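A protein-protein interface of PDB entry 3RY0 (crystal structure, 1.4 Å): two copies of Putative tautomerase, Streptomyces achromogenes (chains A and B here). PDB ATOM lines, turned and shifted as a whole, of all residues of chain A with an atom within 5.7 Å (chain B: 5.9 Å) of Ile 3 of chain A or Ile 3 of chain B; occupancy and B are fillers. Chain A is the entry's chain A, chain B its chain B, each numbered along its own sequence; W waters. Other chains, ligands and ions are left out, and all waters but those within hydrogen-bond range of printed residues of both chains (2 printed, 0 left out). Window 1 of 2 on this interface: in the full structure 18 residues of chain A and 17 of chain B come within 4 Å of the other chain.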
ATOM      1  N   PRO A   1      15.060   8.068   0.286  1.00  0.00           N
ATOM      2  CA  PRO A   1      15.968   7.511  -0.782  1.00  0.00           C
ATOM      3  C   PRO A   1      16.335   8.575  -1.799  1.00  0.00           C
ATOM      4  O   PRO A   1      15.647   9.608  -1.949  1.00  0.00           O
ATOM      5  CB  PRO A   1      15.159   6.397  -1.397  1.00  0.00           C
ATOM      6  CG  PRO A   1      13.886   6.272  -0.630  1.00  0.00           C
ATOM      7  CD  PRO A   1      13.757   7.373   0.335  1.00  0.00           C
ATOM      8  N   LEU A   2      17.405   8.342  -2.581  1.00  0.00           N
ATOM      9  CA  LEU A   2      17.903   9.212  -3.595  1.00  0.00           C
ATOM     10  C   LEU A   2      17.814   8.550  -4.940  1.00  0.00           C
ATOM     11  O   LEU A   2      18.353   7.432  -5.115  1.00  0.00           O
ATOM     12  CB  LEU A   2      19.455   9.666  -3.356  1.00  0.00           C
ATOM     13  CG  LEU A   2      19.953  10.567  -4.545  1.00  0.00           C
ATOM     14  CD1 LEU A   2      19.238  11.901  -4.633  1.00  0.00           C
ATOM     15  CD2 LEU A   2      21.510  10.921  -4.707  1.00  0.00           C
ATOM     16  N   ILE A   3      17.186   9.196  -5.867  1.00  0.00           N
ATOM     17  CA  ILE A   3      17.048   8.659  -7.227  1.00  0.00           C
ATOM     18  C   ILE A   3      17.811   9.561  -8.198  1.00  0.00           C
ATOM     19  O   ILE A   3      17.466  10.763  -8.321  1.00  0.00           O
ATOM     20  CB  ILE A   3      15.552   8.586  -7.646  1.00  0.00           C
ATOM     21  CG1 ILE A   3      14.821   7.666  -6.726  1.00  0.00           C
ATOM     22  CG2 ILE A   3      15.428   8.083  -9.110  1.00  0.00           C
ATOM     23  CD1 ILE A   3      13.238   7.733  -6.909  1.00  0.00           C
ATOM     24  N   ARG A   4      18.853   9.067  -8.852  1.00  0.00           N
ATOM     25  CA  ARG A   4      19.641   9.893  -9.782  1.00  0.00           C
ATOM     26  C   ARG A   4      19.340   9.360 -11.154  1.00  0.00           C
ATOM     27  O   ARG A   4      19.633   8.185 -11.432  1.00  0.00           O
ATOM     28  CB  ARG A   4      21.135   9.782  -9.515  1.00  0.00           C
ATOM     29  CG  ARG A   4      21.916  10.867 -10.211  1.00  0.00           C
ATOM     30  CD  ARG A   4      23.416  11.017  -9.626  1.00  0.00           C
ATOM     31  NE  ARG A   4      23.682  12.473  -9.464  1.00  0.00           N
ATOM     32  CZ  ARG A   4      23.953  13.194  -8.354  1.00  0.00           C
ATOM     33  NH1 ARG A   4      24.115  14.471  -8.582  1.00  0.00           N
ATOM     34  NH2 ARG A   4      24.212  12.756  -7.036  1.00  0.00           N
ATOM     35  N   VAL A   5      18.848  10.221 -12.038  1.00  0.00           N
ATOM     36  CA  VAL A   5      18.489   9.793 -13.378  1.00  0.00           C
ATOM     37  C   VAL A   5      19.494  10.398 -14.347  1.00  0.00           C
ATOM     38  O   VAL A   5      19.795  11.624 -14.264  1.00  0.00           O
ATOM     39  CB  VAL A   5      17.105  10.325 -13.754  1.00  0.00           C
ATOM     40  CG1 VAL A   5      16.643   9.925 -15.179  1.00  0.00           C
ATOM     41  CG2 VAL A   5      16.114   9.955 -12.719  1.00  0.00           C
ATOM     42  N   THR A   6      19.972   9.591 -15.295  1.00  0.00           N
ATOM     43  CA  THR A   6      20.811  10.150 -16.353  1.00  0.00           C
ATOM     44  C   THR A   6      20.041   9.998 -17.697  1.00  0.00           C
ATOM     45  O   THR A   6      19.707   8.877 -18.059  1.00  0.00           O
ATOM     46  CB  THR A   6      22.114   9.327 -16.405  1.00  0.00           C
ATOM     47  OG1 THR A   6      22.769   9.336 -15.126  1.00  0.00           O
ATOM     48  CG2 THR A   6      23.113   9.965 -17.428  1.00  0.00           C
ATOM     49  N   LEU A  23       8.560   9.127 -10.772  1.00  0.00           N
ATOM     50  CA  LEU A  23       9.558   8.293 -10.052  1.00  0.00           C
ATOM     51  C   LEU A  23       9.360   8.342  -8.540  1.00  0.00           C
ATOM     52  O   LEU A  23       9.488   7.344  -7.855  1.00  0.00           O
ATOM     53  CB  LEU A  23      10.978   8.774 -10.424  1.00  0.00           C
ATOM     54  CG  LEU A  23      11.367   8.527 -11.878  1.00  0.00           C
ATOM     55  CD1 LEU A  23      12.748   9.207 -12.096  1.00  0.00           C
ATOM     56  CD2 LEU A  23      11.518   7.053 -12.196  1.00  0.00           C
ATOM     57  N   THR A  24       8.952   9.516  -8.098  1.00  0.00           N
ATOM     58  CA  THR A  24       8.672   9.696  -6.656  1.00  0.00           C
ATOM     59  C   THR A  24       7.441   8.855  -6.242  1.00  0.00           C
ATOM     60  O   THR A  24       7.524   8.193  -5.203  1.00  0.00           O
ATOM     61  CB  THR A  24       8.451  11.184  -6.324  1.00  0.00           C
ATOM     62  OG1 THR A  24       9.650  11.907  -6.661  1.00  0.00           O
ATOM     63  CG2 THR A  24       8.089  11.398  -4.852  1.00  0.00           C
ATOM     64  N   ALA A  27       8.508   5.203  -5.971  1.00  0.00           N
ATOM     65  CA  ALA A  27       9.232   4.878  -4.726  1.00  0.00           C
ATOM     66  C   ALA A  27       8.228   4.908  -3.536  1.00  0.00           C
ATOM     67  O   ALA A  27       8.317   3.994  -2.652  1.00  0.00           O
ATOM     68  CB  ALA A  27      10.368   5.905  -4.497  1.00  0.00           C
ATOM     69  N   VAL A  38      11.690  11.393  -0.518  1.00  0.00           N
ATOM     70  CA  VAL A  38      12.308  10.978  -1.813  1.00  0.00           C
ATOM     71  C   VAL A  38      12.839  12.180  -2.531  1.00  0.00           C
ATOM     72  O   VAL A  38      12.150  13.180  -2.712  1.00  0.00           O
ATOM     73  CB  VAL A  38      11.233  10.319  -2.677  1.00  0.00           C
ATOM     74  CG1 VAL A  38      11.794   9.877  -4.042  1.00  0.00           C
ATOM     75  CG2 VAL A  38      10.500   9.183  -1.924  1.00  0.00           C
ATOM     76  N   ARG A  39      14.147  12.046  -2.858  1.00  0.00           N
ATOM     77  CA  ARG A  39      14.795  13.069  -3.676  1.00  0.00           C
ATOM     78  C   ARG A  39      15.148  12.530  -5.037  1.00  0.00           C
ATOM     79  O   ARG A  39      15.605  11.362  -5.132  1.00  0.00           O
ATOM     80  CB  ARG A  39      16.095  13.661  -2.998  1.00  0.00           C
ATOM     81  CG  ARG A  39      15.711  14.513  -1.831  1.00  0.00           C
ATOM     82  CD  ARG A  39      16.974  14.906  -0.933  1.00  0.00           C
ATOM     83  NE  ARG A  39      16.524  15.929  -0.018  1.00  0.00           N
ATOM     84  CZ  ARG A  39      15.722  15.703   0.992  1.00  0.00           C
ATOM     85  NH1 ARG A  39      15.509  14.472   1.415  1.00  0.00           N
ATOM     86  NH2 ARG A  39      15.229  16.755   1.675  1.00  0.00           N
ATOM     87  N   VAL A  40      14.957  13.314  -6.074  1.00  0.00           N
ATOM     88  CA  VAL A  40      15.322  12.924  -7.440  1.00  0.00           C
ATOM     89  C   VAL A  40      16.202  13.994  -8.000  1.00  0.00           C
ATOM     90  O   VAL A  40      15.864  15.230  -7.964  1.00  0.00           O
ATOM     91  CB  VAL A  40      14.054  12.788  -8.344  1.00  0.00           C
ATOM     92  CG1 VAL A  40      14.435  12.227  -9.708  1.00  0.00           C
ATOM     93  CG2 VAL A  40      12.980  11.868  -7.751  1.00  0.00           C
ATOM     94  N   ILE A  41      17.335  13.602  -8.598  1.00  0.00           N
ATOM     95  CA  ILE A  41      18.215  14.513  -9.293  1.00  0.00           C
ATOM     96  C   ILE A  41      18.267  14.042 -10.778  1.00  0.00           C
ATOM     97  O   ILE A  41      18.566  12.839 -11.030  1.00  0.00           O
ATOM     98  CB  ILE A  41      19.679  14.458  -8.752  1.00  0.00           C
ATOM     99  CG1 ILE A  41      19.675  14.714  -7.247  1.00  0.00           C
ATOM    100  CG2 ILE A  41      20.545  15.482  -9.614  1.00  0.00           C
ATOM    101  CD1 ILE A  41      19.521  16.141  -6.819  1.00  0.00           C
ATOM    102  N   VAL A  42      17.969  14.917 -11.699  1.00  0.00           N
ATOM    103  CA  VAL A  42      17.938  14.559 -13.126  1.00  0.00           C
ATOM    104  C   VAL A  42      19.141  15.186 -13.761  1.00  0.00           C
ATOM    105  O   VAL A  42      19.266  16.445 -13.757  1.00  0.00           O
ATOM    106  CB  VAL A  42      16.636  15.003 -13.821  1.00  0.00           C
ATOM    107  CG1 VAL A  42      16.694  14.699 -15.365  1.00  0.00           C
ATOM    108  CG2 VAL A  42      15.425  14.317 -13.272  1.00  0.00           C
ATOM    109  N   PRO B   1      17.370   5.406 -20.737  1.00  0.00           N
ATOM    110  CA  PRO B   1      17.490   6.267 -19.585  1.00  0.00           C
ATOM    111  C   PRO B   1      18.136   5.419 -18.477  1.00  0.00           C
ATOM    112  O   PRO B   1      17.866   4.210 -18.464  1.00  0.00           O
ATOM    113  CB  PRO B   1      15.991   6.548 -19.314  1.00  0.00           C
ATOM    114  CG  PRO B   1      15.438   6.617 -20.680  1.00  0.00           C
ATOM    115  CD  PRO B   1      16.105   5.634 -21.462  1.00  0.00           C
ATOM    116  N   LEU B   2      19.000   5.989 -17.672  1.00  0.00           N
ATOM    117  CA  LEU B   2      19.670   5.233 -16.597  1.00  0.00           C
ATOM    118  C   LEU B   2      19.196   5.713 -15.268  1.00  0.00           C
ATOM    119  O   LEU B   2      19.018   6.964 -15.132  1.00  0.00           O
ATOM    120  CB  LEU B   2      21.215   5.347 -16.702  1.00  0.00           C
ATOM    121  CG  LEU B   2      21.795   5.084 -18.133  1.00  0.00           C
ATOM    122  CD1 LEU B   2      23.303   5.205 -18.005  1.00  0.00           C
ATOM    123  CD2 LEU B   2      21.468   3.674 -18.604  1.00  0.00           C
ATOM    124  N   ILE B   3      18.866   4.871 -14.338  1.00  0.00           N
ATOM    125  CA  ILE B   3      18.326   5.319 -13.039  1.00  0.00           C
ATOM    126  C   ILE B   3      19.127   4.596 -11.960  1.00  0.00           C
ATOM    127  O   ILE B   3      19.233   3.337 -11.958  1.00  0.00           O
ATOM    128  CB  ILE B   3      16.810   4.984 -12.914  1.00  0.00           C
ATOM    129  CG1 ILE B   3      16.031   5.712 -13.960  1.00  0.00           C
ATOM    130  CG2 ILE B   3      16.355   5.458 -11.481  1.00  0.00           C
ATOM    131  CD1 ILE B   3      14.561   5.219 -14.082  1.00  0.00           C
ATOM    132  N   ARG B   4      19.703   5.353 -11.038  1.00  0.00           N
ATOM    133  CA  ARG B   4      20.348   4.757  -9.837  1.00  0.00           C
ATOM    134  C   ARG B   4      19.567   5.149  -8.612  1.00  0.00           C
ATOM    135  O   ARG B   4      19.361   6.342  -8.333  1.00  0.00           O
ATOM    136  CB  ARG B   4      21.818   5.205  -9.621  1.00  0.00           C
ATOM    137  CG  ARG B   4      22.326   4.670  -8.297  1.00  0.00           C
ATOM    138  CD  ARG B   4      23.712   5.259  -7.910  1.00  0.00           C
ATOM    139  NE  ARG B   4      24.700   4.682  -8.833  1.00  0.00           N
ATOM    140  CZ  ARG B   4      25.492   3.626  -8.592  1.00  0.00           C
ATOM    141  NH1 ARG B   4      26.240   3.144  -9.585  1.00  0.00           N
ATOM    142  NH2 ARG B   4      25.608   3.113  -7.367  1.00  0.00           N
ATOM    143  N   VAL B   5      19.091   4.191  -7.854  1.00  0.00           N
ATOM    144  CA  VAL B   5      18.384   4.496  -6.576  1.00  0.00           C
ATOM    145  C   VAL B   5      19.183   4.039  -5.418  1.00  0.00           C
ATOM    146  O   VAL B   5      19.633   2.829  -5.417  1.00  0.00           O
ATOM    147  CB  VAL B   5      17.101   3.747  -6.464  1.00  0.00           C
ATOM    148  CG1 VAL B   5      16.345   4.117  -5.202  1.00  0.00           C
ATOM    149  CG2 VAL B   5      16.363   3.894  -7.555  1.00  0.00           C
ATOM    150  N   THR B   6      19.494   4.943  -4.523  1.00  0.00           N
ATOM    151  CA  THR B   6      20.256   4.550  -3.321  1.00  0.00           C
ATOM    152  C   THR B   6      19.234   4.617  -2.173  1.00  0.00           C
ATOM    153  O   THR B   6      18.555   5.633  -1.996  1.00  0.00           O
ATOM    154  CB  THR B   6      21.369   5.605  -3.127  1.00  0.00           C
ATOM    155  OG1 THR B   6      22.174   5.682  -4.321  1.00  0.00           O
ATOM    156  CG2 THR B   6      22.278   5.183  -1.924  1.00  0.00           C
ATOM    157  N   LEU B  23       9.750   1.916 -11.112  1.00  0.00           N
ATOM    158  CA  LEU B  23      10.520   3.021 -11.662  1.00  0.00           C
ATOM    159  C   LEU B  23      10.631   2.948 -13.191  1.00  0.00           C
ATOM    160  O   LEU B  23      10.583   3.954 -13.887  1.00  0.00           O
ATOM    161  CB  LEU B  23      11.969   3.021 -11.079  1.00  0.00           C
ATOM    162  CG  LEU B  23      12.036   3.343  -9.580  1.00  0.00           C
ATOM    163  CD1 LEU B  23      13.499   3.109  -9.111  1.00  0.00           C
ATOM    164  CD2 LEU B  23      11.618   4.706  -9.190  1.00  0.00           C
ATOM    165  N   THR B  24      10.691   1.724 -13.716  1.00  0.00           N
ATOM    166  CA  THR B  24      10.739   1.494 -15.125  1.00  0.00           C
ATOM    167  C   THR B  24       9.436   1.939 -15.770  1.00  0.00           C
ATOM    168  O   THR B  24       9.430   2.583 -16.807  1.00  0.00           O
ATOM    169  CB  THR B  24      10.996   0.024 -15.382  1.00  0.00           C
ATOM    170  OG1 THR B  24      12.331  -0.287 -14.935  1.00  0.00           O
ATOM    171  CG2 THR B  24      10.891  -0.255 -16.902  1.00  0.00           C
ATOM    172  N   ALA B  27       9.329   5.798 -15.935  1.00  0.00           N
ATOM    173  CA  ALA B  27      10.085   6.339 -17.072  1.00  0.00           C
ATOM    174  C   ALA B  27       9.444   6.096 -18.459  1.00  0.00           C
ATOM    175  O   ALA B  27       9.342   7.015 -19.255  1.00  0.00           O
ATOM    176  CB  ALA B  27      11.548   5.759 -17.029  1.00  0.00           C
ATOM    177  N   VAL B  38      15.080   1.183 -20.443  1.00  0.00           N
ATOM    178  CA  VAL B  38      15.224   1.758 -19.082  1.00  0.00           C
ATOM    179  C   VAL B  38      16.076   0.780 -18.301  1.00  0.00           C
ATOM    180  O   VAL B  38      15.776  -0.410 -18.194  1.00  0.00           O
ATOM    181  CB  VAL B  38      13.877   1.941 -18.374  1.00  0.00           C
ATOM    182  CG1 VAL B  38      14.154   2.595 -17.039  1.00  0.00           C
ATOM    183  CG2 VAL B  38      12.932   2.877 -19.249  1.00  0.00           C
ATOM    184  N   ARG B  39      17.170   1.292 -17.696  1.00  0.00           N
ATOM    185  CA  ARG B  39      18.068   0.523 -16.915  1.00  0.00           C
ATOM    186  C   ARG B  39      18.156   1.033 -15.501  1.00  0.00           C
ATOM    187  O   ARG B  39      18.334   2.268 -15.369  1.00  0.00           O
ATOM    188  CB  ARG B  39      19.463   0.429 -17.571  1.00  0.00           C
ATOM    189  CG  ARG B  39      19.309  -0.039 -19.051  1.00  0.00           C
ATOM    190  CD  ARG B  39      20.556   0.176 -19.914  1.00  0.00           C
ATOM    191  NE  ARG B  39      21.338  -0.941 -19.574  1.00  0.00           N
ATOM    192  CZ  ARG B  39      21.367  -2.141 -20.143  1.00  0.00           C
ATOM    193  NH1 ARG B  39      20.651  -2.417 -21.236  1.00  0.00           N
ATOM    194  NH2 ARG B  39      22.134  -3.066 -19.539  1.00  0.00           N
ATOM    195  N   VAL B  40      18.011   0.221 -14.484  1.00  0.00           N
ATOM    196  CA  VAL B  40      17.920   0.676 -13.080  1.00  0.00           C
ATOM    197  C   VAL B  40      18.899  -0.109 -12.266  1.00  0.00           C
ATOM    198  O   VAL B  40      18.984  -1.357 -12.344  1.00  0.00           O
ATOM    199  CB  VAL B  40      16.489   0.448 -12.493  1.00  0.00           C
ATOM    200  CG1 VAL B  40      16.387   1.041 -11.055  1.00  0.00           C
ATOM    201  CG2 VAL B  40      15.440   1.108 -13.397  1.00  0.00           C
ATOM    202  N   ILE B  41      19.663   0.586 -11.418  1.00  0.00           N
ATOM    203  CA  ILE B  41      20.533  -0.036 -10.425  1.00  0.00           C
ATOM    204  C   ILE B  41      20.036   0.341  -9.044  1.00  0.00           C
ATOM    205  O   ILE B  41      19.767   1.540  -8.794  1.00  0.00           O
ATOM    206  CB  ILE B  41      22.015   0.451 -10.561  1.00  0.00           C
ATOM    207  CG1 ILE B  41      22.483   0.115 -12.012  1.00  0.00           C
ATOM    208  CG2 ILE B  41      22.901  -0.218  -9.534  1.00  0.00           C
ATOM    209  CD1 ILE B  41      23.975   0.159 -12.252  1.00  0.00           C
ATOM    210  N   VAL B  42      19.871  -0.610  -8.150  1.00  0.00           N
ATOM    211  CA  VAL B  42      19.494  -0.301  -6.763  1.00  0.00           C
ATOM    212  C   VAL B  42      20.702  -0.558  -5.906  1.00  0.00           C
ATOM    213  O   VAL B  42      21.228  -1.691  -5.845  1.00  0.00           O
ATOM    214  CB  VAL B  42      18.336  -1.213  -6.322  1.00  0.00           C
ATOM    215  CG1 VAL B  42      18.053  -1.044  -4.840  1.00  0.00           C
ATOM    216  CG2 VAL B  42      17.144  -0.925  -7.190  1.00  0.00           C
HETATM  217  O   HOH W   1      21.340   7.497  -6.208  1.00  0.00           O
HETATM  218  O   HOH W   2      21.757   7.539 -13.256  1.00  0.00           O
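The backbone carbonyl oxygen of Leu 2 of chain A sits at hydrogen-bond distance from the backbone NH of Thr 6 of chain B.
The backbone NH of Arg 4 of chain A is in hydrogen-bond range of the backbone carbonyl oxygen of Arg 4 of chain B (2.8 Å).
O of Leu 2 of chain B sits at hydrogen-bond distance from N of Thr 6 of chain A, 2.8 Å away.
O of Pro 1 of chain A sits at hydrogen-bond distance from N of Arg 39 of chain A.
N of Ile 3 of chain A lies within hydrogen-bond range of O of Arg 39 of chain A (2.8 Å).
The backbone carbonyl oxygen (O) of Ile 41 of chain A is in hydrogen-bond range of the backbone NH (N) of Val 5 of chain A (2.8 Å).
The backbone carbonyl oxygen (O) of Pro 1 of chain B is in hydrogen-bond range of the backbone NH (N) of Arg 39 of chain B (3.1 Å).
N of Ile 3 of chain B is in hydrogen-bond range of O of Arg 39 of chain B, 2.8 Å away.
O of Ile 3 of chain B lies within hydrogen-bond range of N of Ile 41 of chain B (2.8 Å).
Among the printed residues, merely in contact across the chains: Pro 1 of chain A with Thr 6 of chain B (3.4 Å), Leu 2 of chain A with Arg 4 of chain B (3.5 Å), Leu 2 of chain A with Val 5 of chain B (3.3 Å), Ile 3 of chain A with Ile 3 of chain B (3.7 Å), Ile 3 of chain A with Arg 4 of chain B (3.5 Å), Arg 4 of chain A with Leu 2 of chain B (3.9 Å), Arg 4 of chain A with Ile 3 of chain B (3.5 Å), Val 5 of chain A with Leu 2 of chain B (3.4 Å), Thr 6 of chain A with Pro 1 of chain B (3.7 Å) and Leu 23 of chain A with Leu 23 of chain B (3.6 Å).
Of chain A, only Ile 3 (3.7 Å) and Arg 4 (3.5 Å) come within 4 Å of Ile 3 of chain B.
Printed residues of chain B within 4 Å of Thr 6 of chain A: Pro 1 and Leu 2.
Printed residues of chain A within 4 Å of Arg 4 of chain B: Leu 2, Ile 3 and Arg 4.
Of the printed residues of chain B, Val 5 of chain A touches Leu 2 (3.4 Å).
Of the printed residues of chain B, Leu 23 of chain A touches Leu 23.
Of the printed residues of chain A, Leu 2 of chain B touches Arg 4, Val 5 and Thr 6.
Val 38 of chain A touches none of the printed residues of chain B.
The nearest residue of chain A that does not touch Ile 3 of chain B is Leu 23 of chain A (4.02 Å).
Hydrophobic or aromatic side chains of chain A that line the printed part of chain B: Pro 1, Ile 3, Val 5 and Leu 23.
Among the printed residues, 13 pairs touch across the chains.
Among the printed residues, no Asp or Glu carboxylate lies within 4 Å of a Lys or Arg side-chain nitrogen of the other chain.
Pro 1 of chain A touches Thr 6 of chain B, and with the chains exchanged Thr 6 of chain A touches Pro 1 of chain B.
Leu 2 of chain A touches Arg 4 of chain B, and with the chains exchanged Arg 4 of chain A touches Leu 2 of chain B.
Ile 3 of chain A touches Arg 4 of chain B, and with the chains exchanged Arg 4 of chain A touches Ile 3 of chain B.
Arg 4 of chain B touches its own counterpart, Arg 4 of chain A.
14 positions are printed for both chains.
Of the 13 pairs that touch across the chains among the printed residues, 13 have their exchanged pair printed and touching as well.
Water W1 lies within hydrogen-bond range of the side-chain hydroxyl (OG1) of Thr 6 of chain B (2.7 Å), the backbone carbonyl oxygen (O) of Arg 4 of chain B (3.1 Å) and the backbone carbonyl oxygen (O) of Leu 2 of chain A (3.2 Å).
Water W2 lies within hydrogen-bond range of the side-chain hydroxyl (OG1) of Thr 6 of chain A (2.8 Å), the backbone carbonyl oxygen (O) of Arg 4 of chain A (2.9 Å) and the backbone carbonyl oxygen (O) of Leu 2 of chain B (3.4 Å).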
